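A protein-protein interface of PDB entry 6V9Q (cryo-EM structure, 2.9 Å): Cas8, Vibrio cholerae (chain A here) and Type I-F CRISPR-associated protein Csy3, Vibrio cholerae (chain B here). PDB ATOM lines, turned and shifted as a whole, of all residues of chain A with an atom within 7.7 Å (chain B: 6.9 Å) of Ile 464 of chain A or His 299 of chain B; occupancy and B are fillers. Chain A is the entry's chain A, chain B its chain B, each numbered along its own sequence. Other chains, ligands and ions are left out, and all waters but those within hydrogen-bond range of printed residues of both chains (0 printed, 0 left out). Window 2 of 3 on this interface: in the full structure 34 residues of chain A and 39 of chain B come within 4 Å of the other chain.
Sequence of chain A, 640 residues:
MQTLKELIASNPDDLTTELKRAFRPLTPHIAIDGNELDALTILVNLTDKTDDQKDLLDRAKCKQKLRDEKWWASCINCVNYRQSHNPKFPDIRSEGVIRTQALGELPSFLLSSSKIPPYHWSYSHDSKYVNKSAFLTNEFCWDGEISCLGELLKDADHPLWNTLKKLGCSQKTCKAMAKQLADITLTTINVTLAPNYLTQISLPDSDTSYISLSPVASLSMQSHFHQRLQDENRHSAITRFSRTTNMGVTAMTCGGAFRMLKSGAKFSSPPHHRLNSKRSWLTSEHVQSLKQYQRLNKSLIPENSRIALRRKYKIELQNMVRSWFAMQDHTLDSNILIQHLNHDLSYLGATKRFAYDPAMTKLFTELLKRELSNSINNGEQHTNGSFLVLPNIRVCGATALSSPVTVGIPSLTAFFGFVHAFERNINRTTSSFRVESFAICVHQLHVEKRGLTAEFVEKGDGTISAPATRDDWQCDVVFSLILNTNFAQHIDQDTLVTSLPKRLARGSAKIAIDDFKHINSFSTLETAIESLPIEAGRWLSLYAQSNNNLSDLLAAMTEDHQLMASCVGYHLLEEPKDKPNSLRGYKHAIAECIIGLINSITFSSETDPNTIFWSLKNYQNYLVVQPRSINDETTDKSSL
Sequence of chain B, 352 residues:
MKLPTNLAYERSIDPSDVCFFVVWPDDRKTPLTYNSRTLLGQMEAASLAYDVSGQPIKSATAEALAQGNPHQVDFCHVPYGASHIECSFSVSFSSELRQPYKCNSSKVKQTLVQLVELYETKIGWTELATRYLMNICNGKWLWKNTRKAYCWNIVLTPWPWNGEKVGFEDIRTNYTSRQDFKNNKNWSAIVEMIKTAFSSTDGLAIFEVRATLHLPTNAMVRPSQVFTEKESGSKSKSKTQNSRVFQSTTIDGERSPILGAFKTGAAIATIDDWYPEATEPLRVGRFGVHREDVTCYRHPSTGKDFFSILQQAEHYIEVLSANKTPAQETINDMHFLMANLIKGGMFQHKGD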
ATOM      1  N   GLU A 455     -10.118 -32.023  17.860  1.00  0.00           N
ATOM      2  CA  GLU A 455     -11.019 -31.506  18.875  1.00  0.00           C
ATOM      3  C   GLU A 455     -10.461 -30.241  19.501  1.00  0.00           C
ATOM      4  O   GLU A 455      -9.296 -29.894  19.303  1.00  0.00           O
ATOM      5  CB  GLU A 455     -11.249 -32.552  19.949  1.00  0.00           C
ATOM      6  CG  GLU A 455     -12.089 -33.692  19.482  1.00  0.00           C
ATOM      7  CD  GLU A 455     -12.265 -34.727  20.548  1.00  0.00           C
ATOM      8  OE1 GLU A 455     -11.521 -34.691  21.549  1.00  0.00           O
ATOM      9  OE2 GLU A 455     -13.185 -35.547  20.404  1.00  0.00           O
ATOM     10  N   PHE A 456     -11.300 -29.557  20.271  1.00  0.00           N
ATOM     11  CA  PHE A 456     -10.891 -28.322  20.918  1.00  0.00           C
ATOM     12  C   PHE A 456      -9.971 -28.613  22.095  1.00  0.00           C
ATOM     13  O   PHE A 456     -10.175 -29.570  22.843  1.00  0.00           O
ATOM     14  CB  PHE A 456     -12.121 -27.544  21.378  1.00  0.00           C
ATOM     15  CG  PHE A 456     -12.946 -27.006  20.251  1.00  0.00           C
ATOM     16  CD1 PHE A 456     -12.656 -25.783  19.684  1.00  0.00           C
ATOM     17  CD2 PHE A 456     -13.997 -27.739  19.737  1.00  0.00           C
ATOM     18  CE1 PHE A 456     -13.406 -25.288  18.645  1.00  0.00           C
ATOM     19  CE2 PHE A 456     -14.750 -27.250  18.691  1.00  0.00           C
ATOM     20  CZ  PHE A 456     -14.450 -26.020  18.147  1.00  0.00           C
ATOM     21  N   VAL A 457      -8.932 -27.790  22.232  1.00  0.00           N
ATOM     22  CA  VAL A 457      -7.922 -27.917  23.273  1.00  0.00           C
ATOM     23  C   VAL A 457      -7.863 -26.576  23.993  1.00  0.00           C
ATOM     24  O   VAL A 457      -8.121 -25.528  23.393  1.00  0.00           O
ATOM     25  CB  VAL A 457      -6.538 -28.306  22.672  1.00  0.00           C
ATOM     26  CG1 VAL A 457      -5.477 -28.551  23.740  1.00  0.00           C
ATOM     27  CG2 VAL A 457      -6.645 -29.530  21.779  1.00  0.00           C
ATOM     28  N   GLU A 458      -7.576 -26.608  25.294  1.00  0.00           N
ATOM     29  CA  GLU A 458      -7.278 -25.391  26.046  1.00  0.00           C
ATOM     30  C   GLU A 458      -6.040 -24.683  25.503  1.00  0.00           C
ATOM     31  O   GLU A 458      -5.633 -23.642  26.016  1.00  0.00           O
ATOM     32  CB  GLU A 458      -7.067 -25.705  27.522  1.00  0.00           C
ATOM     33  CG  GLU A 458      -8.306 -26.137  28.262  1.00  0.00           C
ATOM     34  CD  GLU A 458      -8.014 -26.464  29.710  1.00  0.00           C
ATOM     35  OE1 GLU A 458      -6.824 -26.465  30.086  1.00  0.00           O
ATOM     36  OE2 GLU A 458      -8.968 -26.723  30.473  1.00  0.00           O
ATOM     37  N   THR A 463     -10.081 -19.311  26.518  1.00  0.00           N
ATOM     38  CA  THR A 463      -8.939 -19.825  25.774  1.00  0.00           C
ATOM     39  C   THR A 463      -9.159 -21.266  25.327  1.00  0.00           C
ATOM     40  O   THR A 463      -8.367 -22.146  25.645  1.00  0.00           O
ATOM     41  CB  THR A 463      -7.643 -19.753  26.610  1.00  0.00           C
ATOM     42  OG1 THR A 463      -7.815 -20.478  27.835  1.00  0.00           O
ATOM     43  CG2 THR A 463      -7.279 -18.316  26.919  1.00  0.00           C
ATOM     44  N   ILE A 464     -10.241 -21.503  24.592  1.00  0.00           N
ATOM     45  CA  ILE A 464     -10.555 -22.815  24.037  1.00  0.00           C
ATOM     46  C   ILE A 464     -10.750 -22.666  22.537  1.00  0.00           C
ATOM     47  O   ILE A 464     -11.632 -21.925  22.088  1.00  0.00           O
ATOM     48  CB  ILE A 464     -11.801 -23.429  24.685  1.00  0.00           C
ATOM     49  CG1 ILE A 464     -11.537 -23.756  26.149  1.00  0.00           C
ATOM     50  CG2 ILE A 464     -12.209 -24.677  23.949  1.00  0.00           C
ATOM     51  CD1 ILE A 464     -12.746 -24.207  26.884  1.00  0.00           C
ATOM     52  N   SER A 465      -9.936 -23.378  21.765  1.00  0.00           N
ATOM     53  CA  SER A 465     -10.035 -23.350  20.315  1.00  0.00           C
ATOM     54  C   SER A 465      -9.451 -24.642  19.777  1.00  0.00           C
ATOM     55  O   SER A 465      -9.050 -25.524  20.536  1.00  0.00           O
ATOM     56  CB  SER A 465      -9.313 -22.137  19.722  1.00  0.00           C
ATOM     57  OG  SER A 465      -7.918 -22.215  19.946  1.00  0.00           O
ATOM     58  N   ALA A 466      -9.426 -24.749  18.456  1.00  0.00           N
ATOM     59  CA  ALA A 466      -8.861 -25.921  17.818  1.00  0.00           C
ATOM     60  C   ALA A 466      -7.372 -25.706  17.559  1.00  0.00           C
ATOM     61  O   ALA A 466      -6.920 -24.567  17.421  1.00  0.00           O
ATOM     62  CB  ALA A 466      -9.592 -26.209  16.508  1.00  0.00           C
ATOM     63  N   PRO B 276     -25.427 -27.667  32.352  1.00  0.00           N
ATOM     64  CA  PRO B 276     -26.274 -27.002  33.370  1.00  0.00           C
ATOM     65  C   PRO B 276     -27.511 -26.233  32.883  1.00  0.00           C
ATOM     66  O   PRO B 276     -28.300 -25.807  33.735  1.00  0.00           O
ATOM     67  CB  PRO B 276     -25.297 -26.038  34.056  1.00  0.00           C
ATOM     68  CG  PRO B 276     -23.996 -26.642  33.874  1.00  0.00           C
ATOM     69  CD  PRO B 276     -24.017 -27.263  32.524  1.00  0.00           C
ATOM     70  N   PHE B 287     -15.454 -30.750  27.894  1.00  0.00           N
ATOM     71  CA  PHE B 287     -16.051 -29.404  27.936  1.00  0.00           C
ATOM     72  C   PHE B 287     -17.021 -29.137  26.784  1.00  0.00           C
ATOM     73  O   PHE B 287     -16.926 -28.134  26.081  1.00  0.00           O
ATOM     74  CB  PHE B 287     -14.988 -28.290  28.055  1.00  0.00           C
ATOM     75  CG  PHE B 287     -13.799 -28.411  27.140  1.00  0.00           C
ATOM     76  CD1 PHE B 287     -12.628 -28.981  27.613  1.00  0.00           C
ATOM     77  CD2 PHE B 287     -13.831 -27.941  25.844  1.00  0.00           C
ATOM     78  CE1 PHE B 287     -11.522 -29.095  26.812  1.00  0.00           C
ATOM     79  CE2 PHE B 287     -12.727 -28.069  25.028  1.00  0.00           C
ATOM     80  CZ  PHE B 287     -11.568 -28.639  25.523  1.00  0.00           C
ATOM     81  N   GLY B 288     -18.018 -30.023  26.686  1.00  0.00           N
ATOM     82  CA  GLY B 288     -18.820 -30.305  25.505  1.00  0.00           C
ATOM     83  C   GLY B 288     -19.306 -29.149  24.663  1.00  0.00           C
ATOM     84  O   GLY B 288     -20.143 -28.349  25.083  1.00  0.00           O
ATOM     85  N   VAL B 289     -18.774 -29.072  23.457  1.00  0.00           N
ATOM     86  CA  VAL B 289     -18.928 -27.892  22.631  1.00  0.00           C
ATOM     87  C   VAL B 289     -20.168 -28.047  21.767  1.00  0.00           C
ATOM     88  O   VAL B 289     -20.668 -29.147  21.525  1.00  0.00           O
ATOM     89  CB  VAL B 289     -17.685 -27.636  21.762  1.00  0.00           C
ATOM     90  CG1 VAL B 289     -16.453 -27.563  22.620  1.00  0.00           C
ATOM     91  CG2 VAL B 289     -17.533 -28.700  20.708  1.00  0.00           C
ATOM     92  N   CYS B 296     -19.076 -22.976  24.238  1.00  0.00           N
ATOM     93  CA  CYS B 296     -18.700 -24.149  25.014  1.00  0.00           C
ATOM     94  C   CYS B 296     -19.604 -24.196  26.235  1.00  0.00           C
ATOM     95  O   CYS B 296     -19.365 -23.497  27.223  1.00  0.00           O
ATOM     96  CB  CYS B 296     -17.232 -24.100  25.422  1.00  0.00           C
ATOM     97  SG  CYS B 296     -16.057 -24.203  24.065  1.00  0.00           S
ATOM     98  N   TYR B 297     -20.645 -25.016  26.170  1.00  0.00           N
ATOM     99  CA  TYR B 297     -21.253 -25.479  27.400  1.00  0.00           C
ATOM    100  C   TYR B 297     -20.263 -26.406  28.095  1.00  0.00           C
ATOM    101  O   TYR B 297     -19.359 -26.959  27.461  1.00  0.00           O
ATOM    102  CB  TYR B 297     -22.572 -26.191  27.111  1.00  0.00           C
ATOM    103  CG  TYR B 297     -23.604 -25.298  26.462  1.00  0.00           C
ATOM    104  CD1 TYR B 297     -24.346 -24.403  27.214  1.00  0.00           C
ATOM    105  CD2 TYR B 297     -23.833 -25.350  25.095  1.00  0.00           C
ATOM    106  CE1 TYR B 297     -25.285 -23.585  26.628  1.00  0.00           C
ATOM    107  CE2 TYR B 297     -24.771 -24.535  24.497  1.00  0.00           C
ATOM    108  CZ  TYR B 297     -25.493 -23.656  25.268  1.00  0.00           C
ATOM    109  OH  TYR B 297     -26.431 -22.839  24.679  1.00  0.00           O
ATOM    110  N   ARG B 298     -20.431 -26.554  29.412  1.00  0.00           N
ATOM    111  CA  ARG B 298     -19.482 -27.250  30.294  1.00  0.00           C
ATOM    112  C   ARG B 298     -18.085 -26.640  30.235  1.00  0.00           C
ATOM    113  O   ARG B 298     -17.099 -27.364  30.276  1.00  0.00           O
ATOM    114  CB  ARG B 298     -19.391 -28.754  30.000  1.00  0.00           C
ATOM    115  CG  ARG B 298     -20.643 -29.531  30.221  1.00  0.00           C
ATOM    116  CD  ARG B 298     -20.397 -30.971  29.886  1.00  0.00           C
ATOM    117  NE  ARG B 298     -21.585 -31.787  30.064  1.00  0.00           N
ATOM    118  CZ  ARG B 298     -21.918 -32.357  31.212  1.00  0.00           C
ATOM    119  NH1 ARG B 298     -21.151 -32.193  32.277  1.00  0.00           N
ATOM    120  NH2 ARG B 298     -23.015 -33.088  31.299  1.00  0.00           N
ATOM    121  N   HIS B 299     -17.994 -25.315  30.141  1.00  0.00           N
ATOM    122  CA  HIS B 299     -16.714 -24.620  30.198  1.00  0.00           C
ATOM    123  C   HIS B 299     -16.060 -24.860  31.561  1.00  0.00           C
ATOM    124  O   HIS B 299     -16.762 -25.030  32.559  1.00  0.00           O
ATOM    125  CB  HIS B 299     -16.939 -23.124  29.966  1.00  0.00           C
ATOM    126  CG  HIS B 299     -15.683 -22.317  29.883  1.00  0.00           C
ATOM    127  ND1 HIS B 299     -14.882 -22.302  28.765  1.00  0.00           N
ATOM    128  CD2 HIS B 299     -15.075 -21.517  30.788  1.00  0.00           C
ATOM    129  CE1 HIS B 299     -13.842 -21.516  28.978  1.00  0.00           C
ATOM    130  NE2 HIS B 299     -13.934 -21.028  30.200  1.00  0.00           N
ATOM    131  N   PRO B 300     -14.721 -24.920  31.628  1.00  0.00           N
ATOM    132  CA  PRO B 300     -14.051 -25.208  32.912  1.00  0.00           C
ATOM    133  C   PRO B 300     -14.284 -24.192  34.025  1.00  0.00           C
ATOM    134  O   PRO B 300     -13.986 -24.510  35.182  1.00  0.00           O
ATOM    135  CB  PRO B 300     -12.571 -25.258  32.525  1.00  0.00           C
ATOM    136  CG  PRO B 300     -12.582 -25.682  31.124  1.00  0.00           C
ATOM    137  CD  PRO B 300     -13.785 -25.064  30.499  1.00  0.00           C
ATOM    138  N   SER B 301     -14.811 -23.003  33.732  1.00  0.00           N
ATOM    139  CA  SER B 301     -15.198 -22.094  34.801  1.00  0.00           C
ATOM    140  C   SER B 301     -16.448 -22.580  35.521  1.00  0.00           C
ATOM    141  O   SER B 301     -16.668 -22.226  36.683  1.00  0.00           O
ATOM    142  CB  SER B 301     -15.421 -20.691  34.244  1.00  0.00           C
ATOM    143  OG  SER B 301     -16.557 -20.656  33.397  1.00  0.00           O
ATOM    144  N   THR B 302     -17.278 -23.379  34.848  1.00  0.00           N
ATOM    145  CA  THR B 302     -18.435 -23.972  35.511  1.00  0.00           C
ATOM    146  C   THR B 302     -18.003 -25.043  36.503  1.00  0.00           C
ATOM    147  O   THR B 302     -18.601 -25.178  37.575  1.00  0.00           O
ATOM    148  CB  THR B 302     -19.385 -24.567  34.470  1.00  0.00           C
ATOM    149  OG1 THR B 302     -19.678 -23.582  33.474  1.00  0.00           O
ATOM    150  CG2 THR B 302     -20.692 -24.998  35.111  1.00  0.00           C
ATOM    151  N   GLY B 303     -16.945 -25.776  36.186  1.00  0.00           N
ATOM    152  CA  GLY B 303     -16.531 -26.899  36.992  1.00  0.00           C
ATOM    153  C   GLY B 303     -17.162 -28.210  36.598  1.00  0.00           C
ATOM    154  O   GLY B 303     -17.059 -29.179  37.356  1.00  0.00           O
ATOM    155  N   LYS B 304     -17.810 -28.271  35.438  1.00  0.00           N
ATOM    156  CA  LYS B 304     -18.484 -29.473  34.976  1.00  0.00           C
ATOM    157  C   LYS B 304     -17.969 -29.924  33.615  1.00  0.00           C
ATOM    158  O   LYS B 304     -18.698 -30.557  32.852  1.00  0.00           O
ATOM    159  CB  LYS B 304     -19.994 -29.264  34.938  1.00  0.00           C
ATOM    160  CG  LYS B 304     -20.617 -29.183  36.311  1.00  0.00           C
ATOM    161  CD  LYS B 304     -22.101 -28.936  36.215  1.00  0.00           C
ATOM    162  CE  LYS B 304     -22.812 -30.167  35.692  1.00  0.00           C
ATOM    163  NZ  LYS B 304     -24.290 -30.005  35.696  1.00  0.00           N
ATOM    164  N   ASP B 305     -16.719 -29.603  33.296  1.00  0.00           N
ATOM    165  CA  ASP B 305     -16.037 -30.276  32.205  1.00  0.00           C
ATOM    166  C   ASP B 305     -15.520 -31.630  32.680  1.00  0.00           C
ATOM    167  O   ASP B 305     -15.703 -32.022  33.831  1.00  0.00           O
ATOM    168  CB  ASP B 305     -14.907 -29.410  31.653  1.00  0.00           C
ATOM    169  CG  ASP B 305     -13.972 -28.930  32.725  1.00  0.00           C
ATOM    170  OD1 ASP B 305     -14.308 -29.076  33.907  1.00  0.00           O
ATOM    171  OD2 ASP B 305     -12.886 -28.423  32.396  1.00  0.00           O
ATOM    172  N   SER B 308     -12.721 -31.787  35.590  1.00  0.00           N
ATOM    173  CA  SER B 308     -13.158 -31.454  36.938  1.00  0.00           C
ATOM    174  C   SER B 308     -14.024 -32.538  37.558  1.00  0.00           C
ATOM    175  O   SER B 308     -14.463 -32.384  38.700  1.00  0.00           O
ATOM    176  CB  SER B 308     -13.916 -30.132  36.935  1.00  0.00           C
ATOM    177  OG  SER B 308     -13.068 -29.074  36.532  1.00  0.00           O
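Printed residues of chain B within 4 Å of Glu 458 of chain A: Pro 300.
Printed residues of chain A within 4 Å of Pro 300 of chain B: Glu 458 (3.8 Å) and Ile 464 (3.9 Å).
Printed residues of chain A within 4 Å of Cys 296 of chain B: Ile 464.
Val 457 of chain A touches none of the printed residues of chain B.
The side-chain hydroxyl (OG1) of Thr 302 of chain B lies close to the backbone carbonyl oxygen (O) of His 299 of chain B, 3.4 Å away.
Phe 456 of chain A touches Phe 287 of chain B (O to CZ, 3.2 Å).
Phe 456 of chain A touches Val 289 of chain B.
Glu 458 of chain A touches Pro 300 of chain B.
Phe 287 of chain B touches Ile 464 of chain A (CE2 to CG2, 3.6 Å).
Ile 464 of chain A touches Cys 296 of chain B (CG2 to SG, 3.9 Å).
Ile 464 of chain A touches His 299 of chain B.
CD1 of Ile 464 of chain A touches CD of Pro 300 of chain B, at 3.9 Å.
Of the 8 printed residues of chain A, 3 touch a printed residue of chain B.
Hydrophobic or aromatic side chains of chain A that line the printed part of chain B: Phe 456 and Ile 464.
Along chain B the printed residues that touch a printed residue of chain A span positions 287 to 300.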
